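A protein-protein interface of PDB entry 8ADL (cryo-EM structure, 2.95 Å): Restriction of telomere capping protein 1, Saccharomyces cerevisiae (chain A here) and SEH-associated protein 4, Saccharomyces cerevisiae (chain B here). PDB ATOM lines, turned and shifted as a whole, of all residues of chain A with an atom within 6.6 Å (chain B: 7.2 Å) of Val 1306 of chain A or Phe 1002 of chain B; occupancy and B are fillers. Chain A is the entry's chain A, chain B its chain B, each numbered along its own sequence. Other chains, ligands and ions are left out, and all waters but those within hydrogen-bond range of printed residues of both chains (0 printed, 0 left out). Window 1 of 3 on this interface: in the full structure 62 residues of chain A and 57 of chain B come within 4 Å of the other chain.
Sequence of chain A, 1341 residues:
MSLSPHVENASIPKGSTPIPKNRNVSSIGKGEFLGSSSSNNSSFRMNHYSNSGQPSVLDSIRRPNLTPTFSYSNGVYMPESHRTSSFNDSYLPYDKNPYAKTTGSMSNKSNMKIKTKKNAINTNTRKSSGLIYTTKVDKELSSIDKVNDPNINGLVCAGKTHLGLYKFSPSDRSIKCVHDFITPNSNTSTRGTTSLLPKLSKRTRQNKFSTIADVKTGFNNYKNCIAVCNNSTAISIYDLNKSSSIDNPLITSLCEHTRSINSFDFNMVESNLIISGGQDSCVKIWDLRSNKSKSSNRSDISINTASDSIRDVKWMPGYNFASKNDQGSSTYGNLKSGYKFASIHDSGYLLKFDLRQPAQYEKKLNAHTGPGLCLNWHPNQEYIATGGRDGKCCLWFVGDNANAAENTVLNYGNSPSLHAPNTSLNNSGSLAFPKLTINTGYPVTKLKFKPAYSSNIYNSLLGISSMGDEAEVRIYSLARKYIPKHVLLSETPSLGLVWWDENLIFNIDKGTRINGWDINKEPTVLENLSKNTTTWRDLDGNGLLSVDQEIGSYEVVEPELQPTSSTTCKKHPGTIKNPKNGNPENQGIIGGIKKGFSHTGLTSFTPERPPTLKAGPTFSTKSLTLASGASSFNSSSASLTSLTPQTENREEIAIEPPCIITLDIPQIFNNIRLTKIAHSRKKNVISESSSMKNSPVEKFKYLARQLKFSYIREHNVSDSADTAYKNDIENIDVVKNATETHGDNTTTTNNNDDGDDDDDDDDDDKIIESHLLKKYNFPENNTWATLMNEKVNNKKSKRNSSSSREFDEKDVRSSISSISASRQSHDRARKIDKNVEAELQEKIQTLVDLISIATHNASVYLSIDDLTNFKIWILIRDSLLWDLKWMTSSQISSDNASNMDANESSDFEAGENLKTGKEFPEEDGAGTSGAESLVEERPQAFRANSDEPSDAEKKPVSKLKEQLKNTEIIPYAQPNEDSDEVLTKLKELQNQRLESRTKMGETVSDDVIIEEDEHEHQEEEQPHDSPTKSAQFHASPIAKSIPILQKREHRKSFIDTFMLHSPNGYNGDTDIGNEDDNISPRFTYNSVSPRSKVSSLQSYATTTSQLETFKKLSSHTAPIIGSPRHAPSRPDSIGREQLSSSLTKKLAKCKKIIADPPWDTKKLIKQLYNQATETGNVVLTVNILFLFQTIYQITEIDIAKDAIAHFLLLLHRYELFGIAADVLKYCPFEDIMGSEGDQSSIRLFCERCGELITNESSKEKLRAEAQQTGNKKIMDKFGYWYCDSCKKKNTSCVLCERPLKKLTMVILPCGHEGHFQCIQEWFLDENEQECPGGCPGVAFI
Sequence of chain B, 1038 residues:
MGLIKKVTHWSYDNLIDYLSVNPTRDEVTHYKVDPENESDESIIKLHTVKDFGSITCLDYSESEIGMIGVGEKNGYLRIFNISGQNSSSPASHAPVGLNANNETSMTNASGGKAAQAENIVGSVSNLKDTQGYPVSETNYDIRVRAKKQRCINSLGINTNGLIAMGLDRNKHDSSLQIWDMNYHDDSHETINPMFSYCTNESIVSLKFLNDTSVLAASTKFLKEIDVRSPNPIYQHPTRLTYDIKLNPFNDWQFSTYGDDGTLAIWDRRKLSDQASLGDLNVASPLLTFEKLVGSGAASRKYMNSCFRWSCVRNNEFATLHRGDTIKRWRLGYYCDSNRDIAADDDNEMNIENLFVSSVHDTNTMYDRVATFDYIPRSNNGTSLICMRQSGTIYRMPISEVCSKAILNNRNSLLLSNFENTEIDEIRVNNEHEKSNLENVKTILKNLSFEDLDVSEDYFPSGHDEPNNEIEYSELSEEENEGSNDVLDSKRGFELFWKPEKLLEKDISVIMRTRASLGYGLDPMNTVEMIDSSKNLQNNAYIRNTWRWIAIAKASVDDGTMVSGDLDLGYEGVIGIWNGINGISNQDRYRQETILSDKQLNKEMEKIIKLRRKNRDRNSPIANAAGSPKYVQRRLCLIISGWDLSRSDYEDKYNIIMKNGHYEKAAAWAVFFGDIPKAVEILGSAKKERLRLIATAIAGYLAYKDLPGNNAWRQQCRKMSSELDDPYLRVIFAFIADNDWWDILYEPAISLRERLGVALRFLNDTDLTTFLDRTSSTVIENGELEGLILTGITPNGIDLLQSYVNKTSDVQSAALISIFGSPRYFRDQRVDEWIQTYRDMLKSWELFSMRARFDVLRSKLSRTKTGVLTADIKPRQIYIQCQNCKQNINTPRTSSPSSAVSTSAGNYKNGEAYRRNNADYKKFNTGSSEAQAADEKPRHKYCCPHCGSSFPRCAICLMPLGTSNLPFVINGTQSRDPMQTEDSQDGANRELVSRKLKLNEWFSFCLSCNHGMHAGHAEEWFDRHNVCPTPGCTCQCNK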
ATOM      1  N   ILE A1242     -24.908  -8.919 -14.755  1.00  0.00           N
ATOM      2  CA  ILE A1242     -25.719  -9.347 -15.889  1.00  0.00           C
ATOM      3  C   ILE A1242     -26.366 -10.668 -15.499  1.00  0.00           C
ATOM      4  O   ILE A1242     -25.741 -11.731 -15.602  1.00  0.00           O
ATOM      5  CB  ILE A1242     -24.890  -9.494 -17.167  1.00  0.00           C
ATOM      6  CG1 ILE A1242     -24.188  -8.180 -17.488  1.00  0.00           C
ATOM      7  CG2 ILE A1242     -25.774  -9.901 -18.334  1.00  0.00           C
ATOM      8  CD1 ILE A1242     -23.007  -8.354 -18.372  1.00  0.00           C
ATOM      9  N   LEU A1244     -28.972 -13.669 -16.164  1.00  0.00           N
ATOM     10  CA  LEU A1244     -29.456 -14.310 -17.374  1.00  0.00           C
ATOM     11  C   LEU A1244     -30.603 -15.258 -17.062  1.00  0.00           C
ATOM     12  O   LEU A1244     -30.662 -15.858 -15.985  1.00  0.00           O
ATOM     13  CB  LEU A1244     -28.338 -15.085 -18.075  1.00  0.00           C
ATOM     14  CG  LEU A1244     -27.064 -14.323 -18.427  1.00  0.00           C
ATOM     15  CD1 LEU A1244     -25.990 -15.292 -18.884  1.00  0.00           C
ATOM     16  CD2 LEU A1244     -27.341 -13.287 -19.498  1.00  0.00           C
ATOM     17  N   THR A1304     -16.516 -14.710 -22.067  1.00  0.00           N
ATOM     18  CA  THR A1304     -17.244 -14.893 -23.312  1.00  0.00           C
ATOM     19  C   THR A1304     -17.158 -13.631 -24.159  1.00  0.00           C
ATOM     20  O   THR A1304     -16.524 -12.644 -23.785  1.00  0.00           O
ATOM     21  CB  THR A1304     -18.714 -15.231 -23.055  1.00  0.00           C
ATOM     22  OG1 THR A1304     -19.406 -14.051 -22.631  1.00  0.00           O
ATOM     23  CG2 THR A1304     -18.844 -16.289 -21.991  1.00  0.00           C
ATOM     24  N   MET A1305     -17.832 -13.670 -25.310  1.00  0.00           N
ATOM     25  CA  MET A1305     -17.900 -12.519 -26.210  1.00  0.00           C
ATOM     26  C   MET A1305     -19.258 -12.589 -26.904  1.00  0.00           C
ATOM     27  O   MET A1305     -19.420 -13.323 -27.883  1.00  0.00           O
ATOM     28  CB  MET A1305     -16.748 -12.530 -27.205  1.00  0.00           C
ATOM     29  CG  MET A1305     -16.430 -11.174 -27.809  1.00  0.00           C
ATOM     30  SD  MET A1305     -14.720 -11.093 -28.371  1.00  0.00           S
ATOM     31  CE  MET A1305     -14.772  -9.647 -29.420  1.00  0.00           C
ATOM     32  N   VAL A1306     -20.217 -11.826 -26.394  1.00  0.00           N
ATOM     33  CA  VAL A1306     -21.604 -11.945 -26.826  1.00  0.00           C
ATOM     34  C   VAL A1306     -21.789 -11.237 -28.160  1.00  0.00           C
ATOM     35  O   VAL A1306     -21.399 -10.075 -28.322  1.00  0.00           O
ATOM     36  CB  VAL A1306     -22.549 -11.373 -25.759  1.00  0.00           C
ATOM     37  CG1 VAL A1306     -23.974 -11.299 -26.275  1.00  0.00           C
ATOM     38  CG2 VAL A1306     -22.472 -12.206 -24.504  1.00  0.00           C
ATOM     39  N   ILE A1307     -22.379 -11.943 -29.119  1.00  0.00           N
ATOM     40  CA  ILE A1307     -22.822 -11.341 -30.369  1.00  0.00           C
ATOM     41  C   ILE A1307     -24.203 -10.745 -30.130  1.00  0.00           C
ATOM     42  O   ILE A1307     -25.120 -11.440 -29.680  1.00  0.00           O
ATOM     43  CB  ILE A1307     -22.845 -12.375 -31.504  1.00  0.00           C
ATOM     44  CG1 ILE A1307     -21.535 -13.164 -31.519  1.00  0.00           C
ATOM     45  CG2 ILE A1307     -23.059 -11.690 -32.834  1.00  0.00           C
ATOM     46  CD1 ILE A1307     -21.586 -14.421 -32.353  1.00  0.00           C
ATOM     47  N   LEU A1308     -24.349  -9.447 -30.417  1.00  0.00           N
ATOM     48  CA  LEU A1308     -25.508  -8.707 -29.912  1.00  0.00           C
ATOM     49  C   LEU A1308     -26.828  -9.065 -30.595  1.00  0.00           C
ATOM     50  O   LEU A1308     -27.790  -9.381 -29.871  1.00  0.00           O
ATOM     51  CB  LEU A1308     -25.235  -7.197 -29.964  1.00  0.00           C
ATOM     52  CG  LEU A1308     -24.452  -6.499 -28.842  1.00  0.00           C
ATOM     53  CD1 LEU A1308     -25.208  -6.605 -27.521  1.00  0.00           C
ATOM     54  CD2 LEU A1308     -23.007  -6.978 -28.696  1.00  0.00           C
ATOM     55  N   GLY A1311     -27.494 -13.098 -29.815  1.00  0.00           N
ATOM     56  CA  GLY A1311     -27.321 -13.659 -28.489  1.00  0.00           C
ATOM     57  C   GLY A1311     -26.556 -14.966 -28.430  1.00  0.00           C
ATOM     58  O   GLY A1311     -27.054 -15.954 -27.883  1.00  0.00           O
ATOM     59  N   HIS A1312     -25.348 -14.991 -28.988  1.00  0.00           N
ATOM     60  CA  HIS A1312     -24.497 -16.172 -28.972  1.00  0.00           C
ATOM     61  C   HIS A1312     -23.184 -15.856 -28.273  1.00  0.00           C
ATOM     62  O   HIS A1312     -22.630 -14.765 -28.434  1.00  0.00           O
ATOM     63  CB  HIS A1312     -24.217 -16.682 -30.390  1.00  0.00           C
ATOM     64  CG  HIS A1312     -25.396 -17.329 -31.046  1.00  0.00           C
ATOM     65  ND1 HIS A1312     -25.728 -17.105 -32.363  1.00  0.00           N
ATOM     66  CD2 HIS A1312     -26.321 -18.193 -30.566  1.00  0.00           C
ATOM     67  CE1 HIS A1312     -26.807 -17.802 -32.668  1.00  0.00           C
ATOM     68  NE2 HIS A1312     -27.187 -18.471 -31.595  1.00  0.00           N
ATOM     69  N   GLU A1313     -22.690 -16.817 -27.495  1.00  0.00           N
ATOM     70  CA  GLU A1313     -21.457 -16.650 -26.736  1.00  0.00           C
ATOM     71  C   GLU A1313     -20.251 -16.868 -27.650  1.00  0.00           C
ATOM     72  O   GLU A1313     -20.364 -16.927 -28.877  1.00  0.00           O
ATOM     73  CB  GLU A1313     -21.415 -17.614 -25.553  1.00  0.00           C
ATOM     74  CG  GLU A1313     -22.705 -17.776 -24.773  1.00  0.00           C
ATOM     75  CD  GLU A1313     -22.846 -16.792 -23.640  1.00  0.00           C
ATOM     76  OE1 GLU A1313     -21.904 -16.009 -23.403  1.00  0.00           O
ATOM     77  OE2 GLU A1313     -23.887 -16.835 -22.955  1.00  0.00           O
ATOM     78  N   GLY A1314     -19.072 -16.994 -27.048  1.00  0.00           N
ATOM     79  CA  GLY A1314     -17.863 -17.314 -27.778  1.00  0.00           C
ATOM     80  C   GLY A1314     -16.616 -16.855 -27.054  1.00  0.00           C
ATOM     81  O   GLY A1314     -16.651 -15.850 -26.343  1.00  0.00           O
ATOM     82  N   ILE A1319     -14.059 -15.790 -31.580  1.00  0.00           N
ATOM     83  CA  ILE A1319     -14.788 -14.671 -32.172  1.00  0.00           C
ATOM     84  C   ILE A1319     -13.837 -13.746 -32.923  1.00  0.00           C
ATOM     85  O   ILE A1319     -14.143 -13.287 -34.033  1.00  0.00           O
ATOM     86  CB  ILE A1319     -15.584 -13.930 -31.079  1.00  0.00           C
ATOM     87  CG1 ILE A1319     -16.716 -14.814 -30.555  1.00  0.00           C
ATOM     88  CG2 ILE A1319     -16.149 -12.623 -31.592  1.00  0.00           C
ATOM     89  CD1 ILE A1319     -17.731 -15.192 -31.606  1.00  0.00           C
ATOM     90  N   ARG B 875     -31.024 -19.117 -29.223  1.00  0.00           N
ATOM     91  CA  ARG B 875     -30.446 -18.017 -28.465  1.00  0.00           C
ATOM     92  C   ARG B 875     -29.806 -18.522 -27.179  1.00  0.00           C
ATOM     93  O   ARG B 875     -30.309 -19.445 -26.535  1.00  0.00           O
ATOM     94  CB  ARG B 875     -31.514 -16.970 -28.148  1.00  0.00           C
ATOM     95  CG  ARG B 875     -30.944 -15.610 -27.798  1.00  0.00           C
ATOM     96  CD  ARG B 875     -32.015 -14.544 -27.739  1.00  0.00           C
ATOM     97  NE  ARG B 875     -31.427 -13.214 -27.648  1.00  0.00           N
ATOM     98  CZ  ARG B 875     -31.183 -12.429 -28.689  1.00  0.00           C
ATOM     99  NH1 ARG B 875     -31.471 -12.808 -29.922  1.00  0.00           N
ATOM    100  NH2 ARG B 875     -30.636 -11.234 -28.485  1.00  0.00           N
ATOM    101  N   ILE B 877     -28.297 -15.895 -24.980  1.00  0.00           N
ATOM    102  CA  ILE B 877     -28.314 -14.730 -24.102  1.00  0.00           C
ATOM    103  C   ILE B 877     -29.756 -14.290 -23.886  1.00  0.00           C
ATOM    104  O   ILE B 877     -30.474 -13.991 -24.848  1.00  0.00           O
ATOM    105  CB  ILE B 877     -27.471 -13.583 -24.677  1.00  0.00           C
ATOM    106  CG1 ILE B 877     -25.988 -13.930 -24.606  1.00  0.00           C
ATOM    107  CG2 ILE B 877     -27.756 -12.282 -23.950  1.00  0.00           C
ATOM    108  CD1 ILE B 877     -25.479 -14.026 -23.193  1.00  0.00           C
ATOM    109  N   ILE B 879     -30.823 -11.501 -21.353  1.00  0.00           N
ATOM    110  CA  ILE B 879     -30.403 -10.554 -20.327  1.00  0.00           C
ATOM    111  C   ILE B 879     -31.611 -10.111 -19.513  1.00  0.00           C
ATOM    112  O   ILE B 879     -32.645  -9.717 -20.068  1.00  0.00           O
ATOM    113  CB  ILE B 879     -29.685  -9.356 -20.969  1.00  0.00           C
ATOM    114  CG1 ILE B 879     -28.251  -9.725 -21.337  1.00  0.00           C
ATOM    115  CG2 ILE B 879     -29.671  -8.149 -20.043  1.00  0.00           C
ATOM    116  CD1 ILE B 879     -27.663  -8.843 -22.410  1.00  0.00           C
ATOM    117  N   PHE B 950     -28.373  -1.167 -21.020  1.00  0.00           N
ATOM    118  CA  PHE B 950     -27.736  -2.377 -20.537  1.00  0.00           C
ATOM    119  C   PHE B 950     -26.915  -2.079 -19.281  1.00  0.00           C
ATOM    120  O   PHE B 950     -26.668  -0.914 -18.958  1.00  0.00           O
ATOM    121  CB  PHE B 950     -26.849  -2.959 -21.637  1.00  0.00           C
ATOM    122  CG  PHE B 950     -27.589  -3.814 -22.629  1.00  0.00           C
ATOM    123  CD1 PHE B 950     -28.943  -4.069 -22.477  1.00  0.00           C
ATOM    124  CD2 PHE B 950     -26.931  -4.350 -23.724  1.00  0.00           C
ATOM    125  CE1 PHE B 950     -29.622  -4.846 -23.393  1.00  0.00           C
ATOM    126  CE2 PHE B 950     -27.605  -5.130 -24.642  1.00  0.00           C
ATOM    127  CZ  PHE B 950     -28.951  -5.377 -24.476  1.00  0.00           C
ATOM    128  N   PRO B 951     -26.531  -3.114 -18.523  1.00  0.00           N
ATOM    129  CA  PRO B 951     -25.601  -2.905 -17.406  1.00  0.00           C
ATOM    130  C   PRO B 951     -24.279  -2.302 -17.863  1.00  0.00           C
ATOM    131  O   PRO B 951     -23.782  -2.597 -18.952  1.00  0.00           O
ATOM    132  CB  PRO B 951     -25.407  -4.315 -16.841  1.00  0.00           C
ATOM    133  CG  PRO B 951     -26.680  -5.002 -17.139  1.00  0.00           C
ATOM    134  CD  PRO B 951     -27.202  -4.426 -18.427  1.00  0.00           C
ATOM    135  N   PRO B 959     -22.690   2.474 -20.485  1.00  0.00           N
ATOM    136  CA  PRO B 959     -23.676   1.410 -20.726  1.00  0.00           C
ATOM    137  C   PRO B 959     -23.271   0.540 -21.907  1.00  0.00           C
ATOM    138  O   PRO B 959     -22.890   1.043 -22.967  1.00  0.00           O
ATOM    139  CB  PRO B 959     -24.970   2.180 -21.009  1.00  0.00           C
ATOM    140  CG  PRO B 959     -24.764   3.509 -20.369  1.00  0.00           C
ATOM    141  CD  PRO B 959     -23.306   3.810 -20.544  1.00  0.00           C
ATOM    142  N   LEU B 960     -23.354  -0.773 -21.714  1.00  0.00           N
ATOM    143  CA  LEU B 960     -22.949  -1.722 -22.735  1.00  0.00           C
ATOM    144  C   LEU B 960     -23.990  -1.794 -23.850  1.00  0.00           C
ATOM    145  O   LEU B 960     -25.075  -1.212 -23.771  1.00  0.00           O
ATOM    146  CB  LEU B 960     -22.735  -3.104 -22.122  1.00  0.00           C
ATOM    147  CG  LEU B 960     -21.377  -3.404 -21.489  1.00  0.00           C
ATOM    148  CD1 LEU B 960     -21.493  -4.549 -20.503  1.00  0.00           C
ATOM    149  CD2 LEU B 960     -20.352  -3.725 -22.561  1.00  0.00           C
ATOM    150  N   GLY B 961     -23.640  -2.517 -24.909  1.00  0.00           N
ATOM    151  CA  GLY B 961     -24.553  -2.689 -26.019  1.00  0.00           C
ATOM    152  C   GLY B 961     -24.713  -1.487 -26.917  1.00  0.00           C
ATOM    153  O   GLY B 961     -25.618  -1.477 -27.755  1.00  0.00           O
ATOM    154  N   THR B 962     -23.871  -0.466 -26.771  1.00  0.00           N
ATOM    155  CA  THR B 962     -23.931   0.725 -27.608  1.00  0.00           C
ATOM    156  C   THR B 962     -22.643   0.845 -28.408  1.00  0.00           C
ATOM    157  O   THR B 962     -21.547   0.787 -27.842  1.00  0.00           O
ATOM    158  CB  THR B 962     -24.143   1.988 -26.770  1.00  0.00           C
ATOM    159  OG1 THR B 962     -22.970   2.250 -25.991  1.00  0.00           O
ATOM    160  CG2 THR B 962     -25.339   1.828 -25.844  1.00  0.00           C
ATOM    161  N   LEU B 998     -14.441  -3.810 -33.047  1.00  0.00           N
ATOM    162  CA  LEU B 998     -14.676  -5.051 -32.330  1.00  0.00           C
ATOM    163  C   LEU B 998     -14.379  -4.932 -30.842  1.00  0.00           C
ATOM    164  O   LEU B 998     -14.937  -5.698 -30.044  1.00  0.00           O
ATOM    165  CB  LEU B 998     -13.779  -6.146 -32.929  1.00  0.00           C
ATOM    166  CG  LEU B 998     -13.871  -7.591 -32.450  1.00  0.00           C
ATOM    167  CD1 LEU B 998     -15.131  -8.257 -32.947  1.00  0.00           C
ATOM    168  CD2 LEU B 998     -12.623  -8.385 -32.831  1.00  0.00           C
ATOM    169  N   ASN B 999     -13.538  -3.973 -30.454  1.00  0.00           N
ATOM    170  CA  ASN B 999     -13.199  -3.787 -29.046  1.00  0.00           C
ATOM    171  C   ASN B 999     -14.390  -3.303 -28.221  1.00  0.00           C
ATOM    172  O   ASN B 999     -14.455  -3.574 -27.018  1.00  0.00           O
ATOM    173  CB  ASN B 999     -12.048  -2.790 -28.926  1.00  0.00           C
ATOM    174  CG  ASN B 999     -10.687  -3.428 -29.112  1.00  0.00           C
ATOM    175  OD1 ASN B 999     -10.488  -4.607 -28.823  1.00  0.00           O
ATOM    176  ND2 ASN B 999      -9.754  -2.659 -29.653  1.00  0.00           N
ATOM    177  N   GLU B1000     -15.341  -2.601 -28.837  1.00  0.00           N
ATOM    178  CA  GLU B1000     -16.496  -2.118 -28.080  1.00  0.00           C
ATOM    179  C   GLU B1000     -17.697  -3.060 -28.104  1.00  0.00           C
ATOM    180  O   GLU B1000     -18.804  -2.647 -28.442  1.00  0.00           O
ATOM    181  CB  GLU B1000     -16.899  -0.744 -28.596  1.00  0.00           C
ATOM    182  CG  GLU B1000     -16.803  -0.595 -30.094  1.00  0.00           C
ATOM    183  CD  GLU B1000     -17.189   0.789 -30.553  1.00  0.00           C
ATOM    184  OE1 GLU B1000     -17.530   1.629 -29.696  1.00  0.00           O
ATOM    185  OE2 GLU B1000     -17.139   1.039 -31.774  1.00  0.00           O
ATOM    186  N   TRP B1001     -17.501  -4.330 -27.766  1.00  0.00           N
ATOM    187  CA  TRP B1001     -18.591  -5.301 -27.731  1.00  0.00           C
ATOM    188  C   TRP B1001     -18.941  -5.680 -26.299  1.00  0.00           C
ATOM    189  O   TRP B1001     -18.417  -5.136 -25.323  1.00  0.00           O
ATOM    190  CB  TRP B1001     -18.369  -6.569 -28.565  1.00  0.00           C
ATOM    191  CG  TRP B1001     -18.446  -6.424 -30.058  1.00  0.00           C
ATOM    192  CD1 TRP B1001     -18.803  -5.305 -30.760  1.00  0.00           C
ATOM    193  CD2 TRP B1001     -18.472  -7.506 -30.998  1.00  0.00           C
ATOM    194  NE1 TRP B1001     -18.886  -5.596 -32.100  1.00  0.00           N
ATOM    195  CE2 TRP B1001     -18.700  -6.946 -32.268  1.00  0.00           C
ATOM    196  CE3 TRP B1001     -18.251  -8.875 -30.894  1.00  0.00           C
ATOM    197  CZ2 TRP B1001     -18.715  -7.711 -33.423  1.00  0.00           C
ATOM    198  CZ3 TRP B1001     -18.263  -9.635 -32.040  1.00  0.00           C
ATOM    199  CH2 TRP B1001     -18.510  -9.059 -33.292  1.00  0.00           C
ATOM    200  N   PHE B1002     -19.840  -6.648 -26.202  1.00  0.00           N
ATOM    201  CA  PHE B1002     -20.430  -7.077 -24.946  1.00  0.00           C
ATOM    202  C   PHE B1002     -19.739  -8.371 -24.538  1.00  0.00           C
ATOM    203  O   PHE B1002     -20.006  -9.433 -25.106  1.00  0.00           O
ATOM    204  CB  PHE B1002     -21.931  -7.283 -25.149  1.00  0.00           C
ATOM    205  CG  PHE B1002     -22.728  -7.457 -23.884  1.00  0.00           C
ATOM    206  CD1 PHE B1002     -22.868  -8.706 -23.301  1.00  0.00           C
ATOM    207  CD2 PHE B1002     -23.405  -6.387 -23.328  1.00  0.00           C
ATOM    208  CE1 PHE B1002     -23.623  -8.869 -22.156  1.00  0.00           C
ATOM    209  CE2 PHE B1002     -24.164  -6.547 -22.182  1.00  0.00           C
ATOM    210  CZ  PHE B1002     -24.275  -7.791 -21.602  1.00  0.00           C
ATOM    211  N   SER B1003     -18.849  -8.275 -23.555  1.00  0.00           N
ATOM    212  CA  SER B1003     -18.105  -9.412 -23.033  1.00  0.00           C
ATOM    213  C   SER B1003     -18.357  -9.513 -21.538  1.00  0.00           C
ATOM    214  O   SER B1003     -18.359  -8.499 -20.832  1.00  0.00           O
ATOM    215  CB  SER B1003     -16.607  -9.274 -23.312  1.00  0.00           C
ATOM    216  OG  SER B1003     -15.847 -10.067 -22.418  1.00  0.00           O
ATOM    217  N   PHE B1004     -18.551 -10.733 -21.048  1.00  0.00           N
ATOM    218  CA  PHE B1004     -18.785 -10.919 -19.626  1.00  0.00           C
ATOM    219  C   PHE B1004     -18.323 -12.301 -19.193  1.00  0.00           C
ATOM    220  O   PHE B1004     -18.224 -13.232 -19.996  1.00  0.00           O
ATOM    221  CB  PHE B1004     -20.263 -10.697 -19.283  1.00  0.00           C
ATOM    222  CG  PHE B1004     -21.141 -11.878 -19.558  1.00  0.00           C
ATOM    223  CD1 PHE B1004     -21.426 -12.258 -20.857  1.00  0.00           C
ATOM    224  CD2 PHE B1004     -21.718 -12.582 -18.517  1.00  0.00           C
ATOM    225  CE1 PHE B1004     -22.241 -13.339 -21.111  1.00  0.00           C
ATOM    226  CE2 PHE B1004     -22.538 -13.660 -18.766  1.00  0.00           C
ATOM    227  CZ  PHE B1004     -22.800 -14.039 -20.066  1.00  0.00           C
ATOM    228  N   GLY B1011     -19.794  -7.437 -16.503  1.00  0.00           N
ATOM    229  CA  GLY B1011     -19.639  -7.076 -17.896  1.00  0.00           C
ATOM    230  C   GLY B1011     -18.508  -6.101 -18.159  1.00  0.00           C
ATOM    231  O   GLY B1011     -18.151  -5.285 -17.315  1.00  0.00           O
ATOM    232  N   MET B1012     -17.962  -6.194 -19.368  1.00  0.00           N
ATOM    233  CA  MET B1012     -16.876  -5.337 -19.813  1.00  0.00           C
ATOM    234  C   MET B1012     -16.977  -5.182 -21.321  1.00  0.00           C
ATOM    235  O   MET B1012     -17.616  -5.986 -22.004  1.00  0.00           O
ATOM    236  CB  MET B1012     -15.503  -5.910 -19.442  1.00  0.00           C
ATOM    237  CG  MET B1012     -14.987  -5.514 -18.074  1.00  0.00           C
ATOM    238  SD  MET B1012     -13.779  -6.696 -17.447  1.00  0.00           S
ATOM    239  CE  MET B1012     -14.834  -8.095 -17.075  1.00  0.00           C
ATOM    240  N   HIS B1013     -16.346  -4.136 -21.838  1.00  0.00           N
ATOM    241  CA  HIS B1013     -16.063  -4.100 -23.261  1.00  0.00           C
ATOM    242  C   HIS B1013     -14.941  -5.082 -23.573  1.00  0.00           C
ATOM    243  O   HIS B1013     -14.134  -5.424 -22.706  1.00  0.00           O
ATOM    244  CB  HIS B1013     -15.688  -2.685 -23.697  1.00  0.00           C
ATOM    245  CG  HIS B1013     -16.847  -1.736 -23.717  1.00  0.00           C
ATOM    246  ND1 HIS B1013     -17.022  -0.753 -22.767  1.00  0.00           N
ATOM    247  CD2 HIS B1013     -17.894  -1.625 -24.569  1.00  0.00           C
ATOM    248  CE1 HIS B1013     -18.123  -0.076 -23.035  1.00  0.00           C
ATOM    249  NE2 HIS B1013     -18.672  -0.585 -24.123  1.00  0.00           N
ATOM    250  N   ALA B1014     -14.913  -5.558 -24.822  1.00  0.00           N
ATOM    251  CA  ALA B1014     -13.913  -6.551 -25.213  1.00  0.00           C
ATOM    252  C   ALA B1014     -12.505  -5.974 -25.166  1.00  0.00           C
ATOM    253  O   ALA B1014     -11.579  -6.618 -24.656  1.00  0.00           O
ATOM    254  CB  ALA B1014     -14.227  -7.089 -26.607  1.00  0.00           C
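O of Gly 1314 of chain A is in hydrogen-bond range of N of Met 1305 of chain A (2.7 Å). The guanidinium group (NE) of Arg 875 of chain B is in hydrogen-bond range of the backbone carbonyl oxygen (O) of Ile 877 of chain B (3.1 Å). The backbone carbonyl oxygen (O) of Asn 999 of chain B sits at hydrogen-bond distance from the backbone NH (N) of Ala 1014 of chain B.
Val 1306 of chain A touches just these residues of chain B: Ile 877 (3.7 Å), Phe 1002 (2.7 Å) and Phe 1004 (3.6 Å). Of the printed residues of chain A, Trp 1001 of chain B touches Met 1305 and Ile 1319. Of the printed residues of chain A, Ser 1003 of chain B touches Thr 1304 (3.0 Å). The nearest residue of chain B that does not touch Val 1306 of chain A is Trp 1001 of chain B (4.2 Å). The nearest printed residue of chain A that does not touch Ile 879 of chain B is Leu 1244 of chain A (4.1 Å).
Ile 1242 of chain A touches Phe 1002 of chain B. Ile 1242 of chain A touches Gly 1011 of chain B (CD1 to CA, 3.6 Å). Leu 998 of chain B touches Met 1305 of chain A. Val 1306 of chain A touches Phe 1004 of chain B (CG2 to CE1, 3.6 Å). Arg 875 of chain B touches Leu 1308 of chain A (NH2 to O, 3.7 Å). CD1 of Ile 877 of chain B touches OE2 of Glu 1313 of chain A (3.2 Å). OE1 of Glu 1313 of chain A touches CE1 of Phe 1004 of chain B, 3.5 Å away.
Printed residues of chain A that touch a printed residue of chain B: Ile 1242, Leu 1244, Thr 1304, Met 1305, Val 1306, Leu 1308, Gly 1311, Glu 1313 and Ile 1319. Hydrophobic or aromatic side chains of chain A within 4 Å of the printed part of chain B: Ile 1242, Leu 1244, Met 1305, Val 1306, Leu 1308 and Ile 1319. Of the 20 printed residues of chain B, 10 touch a printed residue of chain A. Hydrophobic or aromatic side chains of chain B that line the printed part of chain A: Ile 877, Ile 879, Leu 998, Trp 1001, Phe 1002, Phe 1004 and Ala 1014. Among the printed residues, no Asp or Glu carboxylate lies within 4 Å of a Lys or Arg side-chain nitrogen of the other chain.
The side-chain hydroxyl (OG) of Ser 1003 of chain B sits at hydrogen-bond distance from the backbone carbonyl oxygen (O) of Thr 1304 of chain A (3.0 Å). The backbone NH (N) of Ile 877 of chain B lies within hydrogen-bond range of the backbone carbonyl oxygen (O) of Gly 1311 of chain A (3.2 Å). The backbone carbonyl oxygen (O) of Phe 1004 of chain B sits at hydrogen-bond distance from the side-chain hydroxyl (OG1) of Thr 1304 of chain A, at 3.0 Å. The backbone carbonyl oxygen (O) of Phe 1002 of chain B lies within hydrogen-bond range of the backbone NH (N) of Val 1306 of chain A (2.7 Å).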
